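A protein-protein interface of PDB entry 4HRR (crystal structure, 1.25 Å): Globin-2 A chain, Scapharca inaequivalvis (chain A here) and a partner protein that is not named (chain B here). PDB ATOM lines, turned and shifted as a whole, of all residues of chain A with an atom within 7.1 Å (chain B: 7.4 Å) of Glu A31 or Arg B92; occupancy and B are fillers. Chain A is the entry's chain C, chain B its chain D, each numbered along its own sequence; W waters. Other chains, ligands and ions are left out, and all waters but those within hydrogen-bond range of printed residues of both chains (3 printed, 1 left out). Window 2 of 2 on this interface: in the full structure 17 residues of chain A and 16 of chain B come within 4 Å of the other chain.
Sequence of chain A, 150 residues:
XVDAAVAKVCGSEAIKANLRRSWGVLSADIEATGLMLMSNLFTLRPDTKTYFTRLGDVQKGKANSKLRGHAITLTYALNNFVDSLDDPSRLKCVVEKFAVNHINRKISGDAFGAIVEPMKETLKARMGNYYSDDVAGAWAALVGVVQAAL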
ATOM      1  N   LEU A  26     -21.054  12.138   0.223  1.00  0.00           N
ATOM      2  CA  LEU A  26     -19.795  11.419   0.074  1.00  0.00           C
ATOM      3  C   LEU A  26     -19.031  11.323   1.399  1.00  0.00           C
ATOM      4  O   LEU A  26     -18.372  10.319   1.674  1.00  0.00           O
ATOM      5  CB  LEU A  26     -18.913  12.068  -0.999  1.00  0.00           C
ATOM      6  CG  LEU A  26     -19.477  12.131  -2.420  1.00  0.00           C
ATOM      7  CD1 LEU A  26     -18.464  12.802  -3.337  1.00  0.00           C
ATOM      8  CD2 LEU A  26     -19.855  10.752  -2.941  1.00  0.00           C
ATOM      9  N   SER A  27     -19.143  12.363   2.222  1.00  0.00           N
ATOM     10  CA  SER A  27     -18.435  12.422   3.487  1.00  0.00           C
ATOM     11  C   SER A  27     -18.991  11.475   4.539  1.00  0.00           C
ATOM     12  O   SER A  27     -18.369  11.303   5.582  1.00  0.00           O
ATOM     13  CB  SER A  27     -18.440  13.848   4.025  1.00  0.00           C
ATOM     14  OG  SER A  27     -19.719  14.203   4.504  1.00  0.00           O
ATOM     15  N   ALA A  28     -20.138  10.842   4.271  1.00  0.00           N
ATOM     16  CA  ALA A  28     -20.616   9.762   5.153  1.00  0.00           C
ATOM     17  C   ALA A  28     -19.595   8.626   5.260  1.00  0.00           C
ATOM     18  O   ALA A  28     -19.608   7.864   6.230  1.00  0.00           O
ATOM     19  CB  ALA A  28     -21.934   9.192   4.651  1.00  0.00           C
ATOM     20  N   ASP A  29     -18.751   8.484   4.242  1.00  0.00           N
ATOM     21  CA  ASP A  29     -17.725   7.447   4.240  1.00  0.00           C
ATOM     22  C   ASP A  29     -16.630   7.836   3.267  1.00  0.00           C
ATOM     23  O   ASP A  29     -16.624   7.440   2.097  1.00  0.00           O
ATOM     24  CB  ASP A  29     -18.330   6.080   3.877  1.00  0.00           C
ATOM     25  CG  ASP A  29     -17.435   4.910   4.279  1.00  0.00           C
ATOM     26  OD1 ASP A  29     -16.196   5.107   4.388  1.00  0.00           O
ATOM     27  OD2 ASP A  29     -17.978   3.783   4.467  1.00  0.00           O
ATOM     28  N   ILE A  30     -15.714   8.648   3.774  1.00  0.00           N
ATOM     29  CA  ILE A  30     -14.631   9.189   2.982  1.00  0.00           C
ATOM     30  C   ILE A  30     -13.829   8.079   2.310  1.00  0.00           C
ATOM     31  O   ILE A  30     -13.565   8.119   1.108  1.00  0.00           O
ATOM     32  CB  ILE A  30     -13.749  10.123   3.854  1.00  0.00           C
ATOM     33  CG1 ILE A  30     -14.480  11.461   4.058  1.00  0.00           C
ATOM     34  CG2 ILE A  30     -12.361  10.328   3.249  1.00  0.00           C
ATOM     35  CD1 ILE A  30     -13.826  12.410   5.039  1.00  0.00           C
ATOM     36  N   GLU A  31     -13.441   7.089   3.094  1.00  0.00           N
ATOM     37  CA  GLU A  31     -12.646   5.985   2.571  1.00  0.00           C
ATOM     38  C   GLU A  31     -13.376   5.201   1.483  1.00  0.00           C
ATOM     39  O   GLU A  31     -12.803   4.906   0.435  1.00  0.00           O
ATOM     40  CB  GLU A  31     -12.283   5.056   3.718  1.00  0.00           C
ATOM     41  CG  GLU A  31     -11.475   3.840   3.345  1.00  0.00           C
ATOM     42  CD  GLU A  31     -11.285   2.957   4.562  1.00  0.00           C
ATOM     43  OE1 GLU A  31     -12.303   2.447   5.078  1.00  0.00           O
ATOM     44  OE2 GLU A  31     -10.137   2.782   5.009  1.00  0.00           O
ATOM     45  N   ALA A  32     -14.639   4.868   1.736  1.00  0.00           N
ATOM     46  CA  ALA A  32     -15.424   4.113   0.761  1.00  0.00           C
ATOM     47  C   ALA A  32     -15.650   4.925  -0.515  1.00  0.00           C
ATOM     48  O   ALA A  32     -15.650   4.371  -1.614  1.00  0.00           O
ATOM     49  CB  ALA A  32     -16.755   3.681   1.343  1.00  0.00           C
ATOM     50  N   THR A  33     -15.841   6.232  -0.378  1.00  0.00           N
ATOM     51  CA  THR A  33     -15.949   7.110  -1.544  1.00  0.00           C
ATOM     52  C   THR A  33     -14.705   7.033  -2.415  1.00  0.00           C
ATOM     53  O   THR A  33     -14.798   6.877  -3.643  1.00  0.00           O
ATOM     54  CB  THR A  33     -16.218   8.564  -1.111  1.00  0.00           C
ATOM     55  OG1 THR A  33     -17.570   8.649  -0.642  1.00  0.00           O
ATOM     56  CG2 THR A  33     -16.002   9.520  -2.254  1.00  0.00           C
ATOM     57  N   GLY A  34     -13.538   7.148  -1.786  1.00  0.00           N
ATOM     58  CA  GLY A  34     -12.290   7.115  -2.538  1.00  0.00           C
ATOM     59  C   GLY A  34     -12.104   5.775  -3.242  1.00  0.00           C
ATOM     60  O   GLY A  34     -11.730   5.721  -4.415  1.00  0.00           O
ATOM     61  N   LEU A  35     -12.363   4.680  -2.530  1.00  0.00           N
ATOM     62  CA  LEU A  35     -12.192   3.348  -3.109  1.00  0.00           C
ATOM     63  C   LEU A  35     -13.173   3.124  -4.263  1.00  0.00           C
ATOM     64  O   LEU A  35     -12.817   2.534  -5.278  1.00  0.00           O
ATOM     65  CB  LEU A  35     -12.350   2.249  -2.039  1.00  0.00           C
ATOM     66  CG  LEU A  35     -11.199   2.195  -1.030  1.00  0.00           C
ATOM     67  CD1 LEU A  35     -11.599   1.385   0.199  1.00  0.00           C
ATOM     68  CD2 LEU A  35      -9.999   1.564  -1.719  1.00  0.00           C
ATOM     69  N   MET A  36     -14.400   3.623  -4.121  1.00  0.00           N
ATOM     70  CA  MET A  36     -15.398   3.475  -5.186  1.00  0.00           C
ATOM     71  C   MET A  36     -15.034   4.331  -6.400  1.00  0.00           C
ATOM     72  O   MET A  36     -15.168   3.907  -7.545  1.00  0.00           O
ATOM     73  CB  MET A  36     -16.803   3.812  -4.678  1.00  0.00           C
ATOM     74  CG  MET A  36     -17.889   3.577  -5.710  1.00  0.00           C
ATOM     75  SD  MET A  36     -19.540   3.716  -5.004  1.00  0.00           S
ATOM     76  CE  MET A  36     -19.711   2.089  -4.287  1.00  0.00           C
ATOM     77  N   LEU A  37     -14.556   5.543  -6.153  1.00  0.00           N
ATOM     78  CA  LEU A  37     -14.120   6.402  -7.244  1.00  0.00           C
ATOM     79  C   LEU A  37     -12.962   5.772  -8.012  1.00  0.00           C
ATOM     80  O   LEU A  37     -12.943   5.779  -9.249  1.00  0.00           O
ATOM     81  CB  LEU A  37     -13.753   7.778  -6.703  1.00  0.00           C
ATOM     82  CG  LEU A  37     -13.261   8.784  -7.751  1.00  0.00           C
ATOM     83  CD1 LEU A  37     -14.241   8.989  -8.896  1.00  0.00           C
ATOM     84  CD2 LEU A  37     -12.979  10.106  -7.061  1.00  0.00           C
ATOM     85  N   LYS A  62      -9.919  -2.275  -1.494  1.00  0.00           N
ATOM     86  CA  LYS A  62      -9.531  -2.014  -0.096  1.00  0.00           C
ATOM     87  C   LYS A  62      -8.379  -2.901   0.399  1.00  0.00           C
ATOM     88  O   LYS A  62      -7.542  -2.453   1.180  1.00  0.00           O
ATOM     89  CB  LYS A  62     -10.739  -2.200   0.824  1.00  0.00           C
ATOM     90  CG  LYS A  62     -10.593  -1.632   2.226  1.00  0.00           C
ATOM     91  CD  LYS A  62     -11.663  -2.237   3.117  1.00  0.00           C
ATOM     92  CE  LYS A  62     -11.932  -1.421   4.366  1.00  0.00           C
ATOM     93  NZ  LYS A  62     -12.754  -0.210   4.102  1.00  0.00           N
ATOM     94  N   ARG A  68      -5.450   1.721  -1.140  1.00  0.00           N
ATOM     95  CA  ARG A  68      -6.293   2.258  -0.081  1.00  0.00           C
ATOM     96  C   ARG A  68      -5.763   3.619   0.403  1.00  0.00           C
ATOM     97  O   ARG A  68      -6.519   4.582   0.550  1.00  0.00           O
ATOM     98  CB  ARG A  68      -6.364   1.246   1.062  1.00  0.00           C
ATOM     99  CG  ARG A  68      -7.246   1.689   2.201  1.00  0.00           C
ATOM    100  CD  ARG A  68      -7.346   0.565   3.212  1.00  0.00           C
ATOM    101  NE  ARG A  68      -8.284   0.907   4.267  1.00  0.00           N
ATOM    102  CZ  ARG A  68      -8.554   0.108   5.291  1.00  0.00           C
ATOM    103  NH1 ARG A  68      -7.932  -1.051   5.405  1.00  0.00           N
ATOM    104  NH2 ARG A  68      -9.449   0.472   6.201  1.00  0.00           N
ATOM    105  N   GLY A  69      -4.465   3.685   0.657  1.00  0.00           N
ATOM    106  CA  GLY A  69      -3.860   4.919   1.125  1.00  0.00           C
ATOM    107  C   GLY A  69      -4.017   6.035   0.095  1.00  0.00           C
ATOM    108  O   GLY A  69      -4.307   7.199   0.433  1.00  0.00           O
ATOM    109  N   ALA A  71      -6.430   6.191  -2.284  1.00  0.00           N
ATOM    110  CA  ALA A  71      -7.837   6.506  -2.398  1.00  0.00           C
ATOM    111  C   ALA A  71      -8.302   7.446  -1.278  1.00  0.00           C
ATOM    112  O   ALA A  71      -9.100   8.344  -1.505  1.00  0.00           O
ATOM    113  CB  ALA A  71      -8.630   5.212  -2.378  1.00  0.00           C
ATOM    114  N   ILE A  72      -7.797   7.225  -0.070  1.00  0.00           N
ATOM    115  CA  ILE A  72      -8.124   8.091   1.063  1.00  0.00           C
ATOM    116  C   ILE A  72      -7.594   9.509   0.821  1.00  0.00           C
ATOM    117  O   ILE A  72      -8.324  10.488   0.956  1.00  0.00           O
ATOM    118  CB  ILE A  72      -7.591   7.491   2.384  1.00  0.00           C
ATOM    119  CG1 ILE A  72      -8.356   6.206   2.714  1.00  0.00           C
ATOM    120  CG2 ILE A  72      -7.700   8.507   3.522  1.00  0.00           C
ATOM    121  CD1 ILE A  72      -7.732   5.393   3.820  1.00  0.00           C
ATOM    122  N   THR A  75      -9.566  11.435  -1.694  1.00  0.00           N
ATOM    123  CA  THR A  75     -10.848  11.904  -1.199  1.00  0.00           C
ATOM    124  C   THR A  75     -10.693  13.152  -0.336  1.00  0.00           C
ATOM    125  O   THR A  75     -11.534  14.044  -0.394  1.00  0.00           O
ATOM    126  CB  THR A  75     -11.621  10.785  -0.478  1.00  0.00           C
ATOM    127  OG1 THR A  75     -11.659   9.624  -1.321  1.00  0.00           O
ATOM    128  CG2 THR A  75     -13.047  11.226  -0.226  1.00  0.00           C
ATOM    129  N   TYR A  76      -9.621  13.244   0.443  1.00  0.00           N
ATOM    130  CA  TYR A  76      -9.345  14.501   1.146  1.00  0.00           C
ATOM    131  C   TYR A  76      -9.003  15.666   0.209  1.00  0.00           C
ATOM    132  O   TYR A  76      -9.225  16.802   0.572  1.00  0.00           O
ATOM    133  CB  TYR A  76      -8.278  14.316   2.238  1.00  0.00           C
ATOM    134  CG  TYR A  76      -8.780  13.507   3.417  1.00  0.00           C
ATOM    135  CD1 TYR A  76      -9.802  13.971   4.230  1.00  0.00           C
ATOM    136  CD2 TYR A  76      -8.243  12.265   3.701  1.00  0.00           C
ATOM    137  CE1 TYR A  76     -10.273  13.216   5.299  1.00  0.00           C
ATOM    138  CE2 TYR A  76      -8.703  11.507   4.758  1.00  0.00           C
ATOM    139  CZ  TYR A  76      -9.720  11.978   5.544  1.00  0.00           C
ATOM    140  OH  TYR A  76     -10.164  11.202   6.580  1.00  0.00           O
ATOM    141  N   ARG A 126     -23.766   6.615  -5.069  1.00  0.00           N
ATOM    142  CA  ARG A 126     -23.734   6.984  -3.656  1.00  0.00           C
ATOM    143  C   ARG A 126     -24.803   8.008  -3.260  1.00  0.00           C
ATOM    144  O   ARG A 126     -25.087   8.142  -2.078  1.00  0.00           O
ATOM    145  CB  ARG A 126     -22.346   7.495  -3.261  1.00  0.00           C
ATOM    146  CG  ARG A 126     -21.226   6.507  -3.518  1.00  0.00           C
ATOM    147  CD  ARG A 126     -19.938   6.889  -2.812  1.00  0.00           C
ATOM    148  NE  ARG A 126     -20.044   6.691  -1.374  1.00  0.00           N
ATOM    149  CZ  ARG A 126     -19.891   5.530  -0.748  1.00  0.00           C
ATOM    150  NH1 ARG A 126     -19.566   4.430  -1.420  1.00  0.00           N
ATOM    151  NH2 ARG A 126     -20.045   5.479   0.566  1.00  0.00           N
ATOM    152  N   VAL B  12      -4.265   2.833  18.026  1.00  0.00           N
ATOM    153  CA  VAL B  12      -5.656   2.403  17.907  1.00  0.00           C
ATOM    154  C   VAL B  12      -6.175   1.868  19.249  1.00  0.00           C
ATOM    155  O   VAL B  12      -7.372   1.908  19.521  1.00  0.00           O
ATOM    156  CB  VAL B  12      -5.807   1.371  16.772  1.00  0.00           C
ATOM    157  CG1 VAL B  12      -7.209   0.771  16.743  1.00  0.00           C
ATOM    158  CG2 VAL B  12      -5.499   2.031  15.439  1.00  0.00           C
ATOM    159  N   GLN B  81      -6.186  15.798   9.322  1.00  0.00           N
ATOM    160  CA  GLN B  81      -7.570  15.256   9.339  1.00  0.00           C
ATOM    161  C   GLN B  81      -7.569  13.771   9.029  1.00  0.00           C
ATOM    162  O   GLN B  81      -8.294  13.000   9.660  1.00  0.00           O
ATOM    163  CB  GLN B  81      -8.435  16.006   8.323  1.00  0.00           C
ATOM    164  CG  GLN B  81      -9.887  15.547   8.275  1.00  0.00           C
ATOM    165  CD  GLN B  81     -10.680  15.948   9.496  1.00  0.00           C
ATOM    166  OE1 GLN B  81     -11.019  17.113   9.674  1.00  0.00           O
ATOM    167  NE2 GLN B  81     -10.977  14.992  10.343  1.00  0.00           N
ATOM    168  N   ASN B  82      -6.771  13.393   8.032  1.00  0.00           N
ATOM    169  CA  ASN B  82      -6.579  11.983   7.642  1.00  0.00           C
ATOM    170  C   ASN B  82      -6.176  11.128   8.875  1.00  0.00           C
ATOM    171  O   ASN B  82      -6.817  10.122   9.190  1.00  0.00           O
ATOM    172  CB  ASN B  82      -5.528  11.982   6.524  1.00  0.00           C
ATOM    173  CG  ASN B  82      -5.462  10.709   5.719  1.00  0.00           C
ATOM    174  OD1 ASN B  82      -5.870   9.641   6.161  1.00  0.00           O
ATOM    175  ND2 ASN B  82      -4.903  10.817   4.521  1.00  0.00           N
ATOM    176  N   PHE B  83      -5.126  11.538   9.578  1.00  0.00           N
ATOM    177  CA  PHE B  83      -4.745  10.874  10.837  1.00  0.00           C
ATOM    178  C   PHE B  83      -5.934  10.757  11.786  1.00  0.00           C
ATOM    179  O   PHE B  83      -6.201   9.684  12.322  1.00  0.00           O
ATOM    180  CB  PHE B  83      -3.657  11.669  11.578  1.00  0.00           C
ATOM    181  CG  PHE B  83      -2.238  11.338  11.216  1.00  0.00           C
ATOM    182  CD1 PHE B  83      -1.787  10.033  11.160  1.00  0.00           C
ATOM    183  CD2 PHE B  83      -1.319  12.371  11.062  1.00  0.00           C
ATOM    184  CE1 PHE B  83      -0.458   9.761  10.890  1.00  0.00           C
ATOM    185  CE2 PHE B  83       0.014  12.100  10.797  1.00  0.00           C
ATOM    186  CZ  PHE B  83       0.441  10.795  10.704  1.00  0.00           C
ATOM    187  N   VAL B  84      -6.632  11.864  12.023  1.00  0.00           N
ATOM    188  CA  VAL B  84      -7.709  11.882  13.006  1.00  0.00           C
ATOM    189  C   VAL B  84      -8.805  10.898  12.615  1.00  0.00           C
ATOM    190  O   VAL B  84      -9.418  10.287  13.485  1.00  0.00           O
ATOM    191  CB  VAL B  84      -8.283  13.298  13.164  1.00  0.00           C
ATOM    192  CG1 VAL B  84      -9.592  13.292  13.940  1.00  0.00           C
ATOM    193  CG2 VAL B  84      -7.262  14.176  13.851  1.00  0.00           C
ATOM    194  N   ASP B  85      -9.047  10.753  11.318  1.00  0.00           N
ATOM    195  CA  ASP B  85     -10.075   9.837  10.824  1.00  0.00           C
ATOM    196  C   ASP B  85      -9.641   8.364  10.770  1.00  0.00           C
ATOM    197  O   ASP B  85     -10.464   7.489  10.504  1.00  0.00           O
ATOM    198  CB  ASP B  85     -10.559  10.295   9.449  1.00  0.00           C
ATOM    199  CG  ASP B  85     -11.391  11.556   9.510  1.00  0.00           C
ATOM    200  OD1 ASP B  85     -11.855  11.947  10.601  1.00  0.00           O
ATOM    201  OD2 ASP B  85     -11.602  12.153   8.451  1.00  0.00           O
ATOM    202  N   ALA B  86      -8.377   8.082  11.066  1.00  0.00           N
ATOM    203  CA  ALA B  86      -7.814   6.729  11.001  1.00  0.00           C
ATOM    204  C   ALA B  86      -7.589   6.076  12.376  1.00  0.00           C
ATOM    205  O   ALA B  86      -7.006   5.000  12.448  1.00  0.00           O
ATOM    206  CB  ALA B  86      -6.493   6.801  10.256  1.00  0.00           C
ATOM    207  N   LEU B  87      -8.079   6.677  13.449  1.00  0.00           N
ATOM    208  CA  LEU B  87      -7.717   6.270  14.801  1.00  0.00           C
ATOM    209  C   LEU B  87      -8.405   4.985  15.273  1.00  0.00           C
ATOM    210  O   LEU B  87      -8.012   4.432  16.288  1.00  0.00           O
ATOM    211  CB  LEU B  87      -8.036   7.382  15.800  1.00  0.00           C
ATOM    212  CG  LEU B  87      -7.276   8.686  15.600  1.00  0.00           C
ATOM    213  CD1 LEU B  87      -7.780   9.722  16.576  1.00  0.00           C
ATOM    214  CD2 LEU B  87      -5.782   8.462  15.758  1.00  0.00           C
ATOM    215  N   ASP B  88      -9.425   4.520  14.550  1.00  0.00           N
ATOM    216  CA  ASP B  88     -10.156   3.311  14.938  1.00  0.00           C
ATOM    217  C   ASP B  88      -9.934   2.118  14.011  1.00  0.00           C
ATOM    218  O   ASP B  88     -10.660   1.134  14.086  1.00  0.00           O
ATOM    219  CB  ASP B  88     -11.644   3.624  14.981  1.00  0.00           C
ATOM    220  CG  ASP B  88     -12.007   4.600  16.075  1.00  0.00           C
ATOM    221  OD1 ASP B  88     -11.344   4.620  17.130  1.00  0.00           O
ATOM    222  OD2 ASP B  88     -12.981   5.338  15.877  1.00  0.00           O
ATOM    223  N   ASP B  89      -8.943   2.194  13.139  1.00  0.00           N
ATOM    224  CA  ASP B  89      -8.743   1.167  12.116  1.00  0.00           C
ATOM    225  C   ASP B  89      -7.251   1.058  11.847  1.00  0.00           C
ATOM    226  O   ASP B  89      -6.676   1.915  11.180  1.00  0.00           O
ATOM    227  CB  ASP B  89      -9.525   1.555  10.854  1.00  0.00           C
ATOM    228  CG  ASP B  89      -9.456   0.497   9.756  1.00  0.00           C
ATOM    229  OD1 ASP B  89      -8.445  -0.233   9.670  1.00  0.00           O
ATOM    230  OD2 ASP B  89     -10.408   0.423   8.946  1.00  0.00           O
ATOM    231  N   VAL B  90      -6.618   0.003  12.357  1.00  0.00           N
ATOM    232  CA  VAL B  90      -5.163  -0.128  12.324  1.00  0.00           C
ATOM    233  C   VAL B  90      -4.624  -0.219  10.908  1.00  0.00           C
ATOM    234  O   VAL B  90      -3.608   0.380  10.589  1.00  0.00           O
ATOM    235  CB  VAL B  90      -4.709  -1.395  13.087  1.00  0.00           C
ATOM    236  CG1 VAL B  90      -3.226  -1.679  12.869  1.00  0.00           C
ATOM    237  CG2 VAL B  90      -5.007  -1.272  14.578  1.00  0.00           C
ATOM    238  N   GLU B  91      -5.286  -1.000  10.060  1.00  0.00           N
ATOM    239  CA  GLU B  91      -4.834  -1.142   8.684  1.00  0.00           C
ATOM    240  C   GLU B  91      -4.999   0.181   7.946  1.00  0.00           C
ATOM    241  O   GLU B  91      -4.165   0.539   7.099  1.00  0.00           O
ATOM    242  CB  GLU B  91      -5.567  -2.254   7.941  1.00  0.00           C
ATOM    243  CG  GLU B  91      -5.241  -3.660   8.430  1.00  0.00           C
ATOM    244  CD  GLU B  91      -3.774  -4.041   8.300  1.00  0.00           C
ATOM    245  OE1 GLU B  91      -3.089  -3.548   7.384  1.00  0.00           O
ATOM    246  OE2 GLU B  91      -3.302  -4.865   9.116  1.00  0.00           O
ATOM    247  N   ARG B  92      -6.080   0.907   8.240  1.00  0.00           N
ATOM    248  CA  ARG B  92      -6.228   2.264   7.707  1.00  0.00           C
ATOM    249  C   ARG B  92      -5.079   3.187   8.145  1.00  0.00           C
ATOM    250  O   ARG B  92      -4.445   3.840   7.317  1.00  0.00           O
ATOM    251  CB  ARG B  92      -7.559   2.861   8.124  1.00  0.00           C
ATOM    252  CG  ARG B  92      -7.787   4.242   7.518  1.00  0.00           C
ATOM    253  CD  ARG B  92      -9.214   4.701   7.757  1.00  0.00           C
ATOM    254  NE  ARG B  92      -9.429   6.086   7.327  1.00  0.00           N
ATOM    255  CZ  ARG B  92     -10.629   6.614   7.111  1.00  0.00           C
ATOM    256  NH1 ARG B  92     -11.725   5.870   7.303  1.00  0.00           N
ATOM    257  NH2 ARG B  92     -10.726   7.879   6.695  1.00  0.00           N
ATOM    258  N   LEU B  93      -4.802   3.226   9.443  1.00  0.00           N
ATOM    259  CA  LEU B  93      -3.727   4.079   9.948  1.00  0.00           C
ATOM    260  C   LEU B  93      -2.378   3.690   9.314  1.00  0.00           C
ATOM    261  O   LEU B  93      -1.601   4.567   8.902  1.00  0.00           O
ATOM    262  CB  LEU B  93      -3.675   3.994  11.474  1.00  0.00           C
ATOM    263  CG  LEU B  93      -2.585   4.853  12.143  1.00  0.00           C
ATOM    264  CD1 LEU B  93      -2.692   6.329  11.778  1.00  0.00           C
ATOM    265  CD2 LEU B  93      -2.641   4.648  13.645  1.00  0.00           C
ATOM    266  N   LYS B  94      -2.116   2.389   9.206  1.00  0.00           N
ATOM    267  CA  LYS B  94      -0.849   1.930   8.645  1.00  0.00           C
ATOM    268  C   LYS B  94      -0.694   2.356   7.189  1.00  0.00           C
ATOM    269  O   LYS B  94       0.362   2.843   6.801  1.00  0.00           O
ATOM    270  CB  LYS B  94      -0.700   0.411   8.776  1.00  0.00           C
ATOM    271  CG  LYS B  94      -0.493  -0.080  10.210  1.00  0.00           C
ATOM    272  CD  LYS B  94      -0.097  -1.544  10.294  1.00  0.00           C
ATOM    273  CE  LYS B  94      -1.176  -2.470   9.766  1.00  0.00           C
ATOM    274  NZ  LYS B  94      -0.960  -3.871  10.234  1.00  0.00           N
ATOM    275  N   CYS B  95      -1.743   2.217   6.383  1.00  0.00           N
ATOM    276  CA  CYS B  95      -1.616   2.592   4.964  1.00  0.00           C
ATOM    277  C   CYS B  95      -1.474   4.108   4.776  1.00  0.00           C
ATOM    278  O   CYS B  95      -0.804   4.573   3.853  1.00  0.00           O
ATOM    279  CB  CYS B  95      -2.736   2.023   4.103  1.00  0.00           C
ATOM    280  SG  CYS B  95      -4.305   2.903   4.047  1.00  0.00           S
ATOM    281  N   VAL B  96      -2.083   4.884   5.668  1.00  0.00           N
ATOM    282  CA  VAL B  96      -1.951   6.341   5.641  1.00  0.00           C
ATOM    283  C   VAL B  96      -0.521   6.756   5.999  1.00  0.00           C
ATOM    284  O   VAL B  96       0.100   7.596   5.333  1.00  0.00           O
ATOM    285  CB  VAL B  96      -2.990   6.971   6.605  1.00  0.00           C
ATOM    286  CG1 VAL B  96      -2.666   8.431   6.899  1.00  0.00           C
ATOM    287  CG2 VAL B  96      -4.388   6.813   6.024  1.00  0.00           C
ATOM    288  N   VAL B  97      -0.006   6.176   7.068  1.00  0.00           N
ATOM    289  CA  VAL B  97       1.359   6.413   7.488  1.00  0.00           C
ATOM    290  C   VAL B  97       2.367   6.022   6.403  1.00  0.00           C
ATOM    291  O   VAL B  97       3.304   6.786   6.105  1.00  0.00           O
ATOM    292  CB  VAL B  97       1.651   5.624   8.781  1.00  0.00           C
ATOM    293  CG1 VAL B  97       3.142   5.444   9.005  1.00  0.00           C
ATOM    294  CG2 VAL B  97       0.981   6.311   9.962  1.00  0.00           C
ATOM    295  N   GLU B  98       2.175   4.852   5.809  1.00  0.00           N
ATOM    296  CA  GLU B  98       3.111   4.374   4.804  1.00  0.00           C
ATOM    297  C   GLU B  98       3.147   5.300   3.612  1.00  0.00           C
ATOM    298  O   GLU B  98       4.217   5.560   3.074  1.00  0.00           O
ATOM    299  CB  GLU B  98       2.770   2.954   4.395  1.00  0.00           C
ATOM    300  CG  GLU B  98       3.190   1.961   5.464  1.00  0.00           C
ATOM    301  CD  GLU B  98       2.545   0.611   5.297  1.00  0.00           C
ATOM    302  OE1 GLU B  98       1.488   0.535   4.643  1.00  0.00           O
ATOM    303  OE2 GLU B  98       3.091  -0.376   5.832  1.00  0.00           O
HETATM  304  O   HOH W   1     -12.688   3.417   7.810  1.00  0.00           O
HETATM  305  O   HOH W   2      -9.128  -2.216   7.850  1.00  0.00           O
HETATM  306  O   HOH W   3      -3.898   8.590   2.789  1.00  0.00           O
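Printed residues of chain B within 4 Å of Glu A31: Arg B92. Of the printed residues of chain B, Gly A69 touches Cys B95 (3.5 Å). Printed residues of chain A within 4 Å of Gln B81: Tyr A76 (3.8 Å). Printed residues of chain A within 4 Å of Glu B91: Arg A68 (3.7 Å). Of chain A, only Glu A31 (3.5 Å), Arg A68 (3.6 Å), Ile A72 (3.9 Å) and Tyr A76 (3.4 Å) come within 4 Å of Arg B92.
Of the 19 printed residues of chain B, 7 touch a printed residue of chain A. Along chain B the printed residues that touch a printed residue of chain A span positions 81 to 95. Among the printed residues, Asp or Glu carboxylates within 4 Å of a Lys or Arg side-chain nitrogen of the other chain: Arg A68 with Asp B89 (2.9 Å).
The backbone NH of Arg B92 lies within hydrogen-bond range of the side-chain carboxylate of Asp B89, at 3.0 Å. NE2 of Gln B81 lies within hydrogen-bond range of OD1 of Asp B85, at 3.2 Å. The side-chain carboxylate of Glu A31 is in salt-bridge range of the side-chain amino group of Lys A62 (2.9 Å). The side-chain amino group (NZ) of Lys B94 is in salt-bridge range of the side-chain carboxylate (OE2) of Glu B91 (2.8 Å). NH2 of Arg A68 lies within salt-bridge range of OE2 of Glu A31, at 2.7 Å. OD1 of Asp B89 lies within hydrogen-bond range of N of Glu B91, at 3.3 Å.
Among the printed residues, merely in contact across the chains: Ile A72 with Asn B82 (3.4 Å), Tyr A76 with Asn B82 (3.5 Å), Glu A31 with Arg B92 (3.5 Å), Arg A68 with Arg B92 (3.6 Å), Arg A68 with Glu B91 (3.7 Å), Arg A68 with Cys B95 (3.7 Å), Tyr A76 with Gln B81 (3.8 Å) and Ile A72 with Arg B92 (3.9 Å).
Water W1 bridges the guanidinium group (NH1) of Arg B92 and the side-chain carboxylate (OE1) of Glu A31. Water W3 lies within hydrogen-bond range of O of Gly A69 (2.8 Å) and ND2 of Asn B82 (3.0 Å). Water W2 bridges OD1 of Asp B89 and NH1 of Arg A68.
OH of Tyr A76 lies within hydrogen-bond range of OD2 of Asp B85 (2.5 Å). OH of Tyr A76 sits at hydrogen-bond distance from NH2 of Arg B92 (3.4 Å). The guanidinium group of Arg A68 is in salt-bridge range of the side-chain carboxylate of Asp B89 (2.9 Å). The backbone NH (N) of Gly A69 is in hydrogen-bond range of the side-chain sulfur (SG) of Cys B95, 3.5 Å away.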
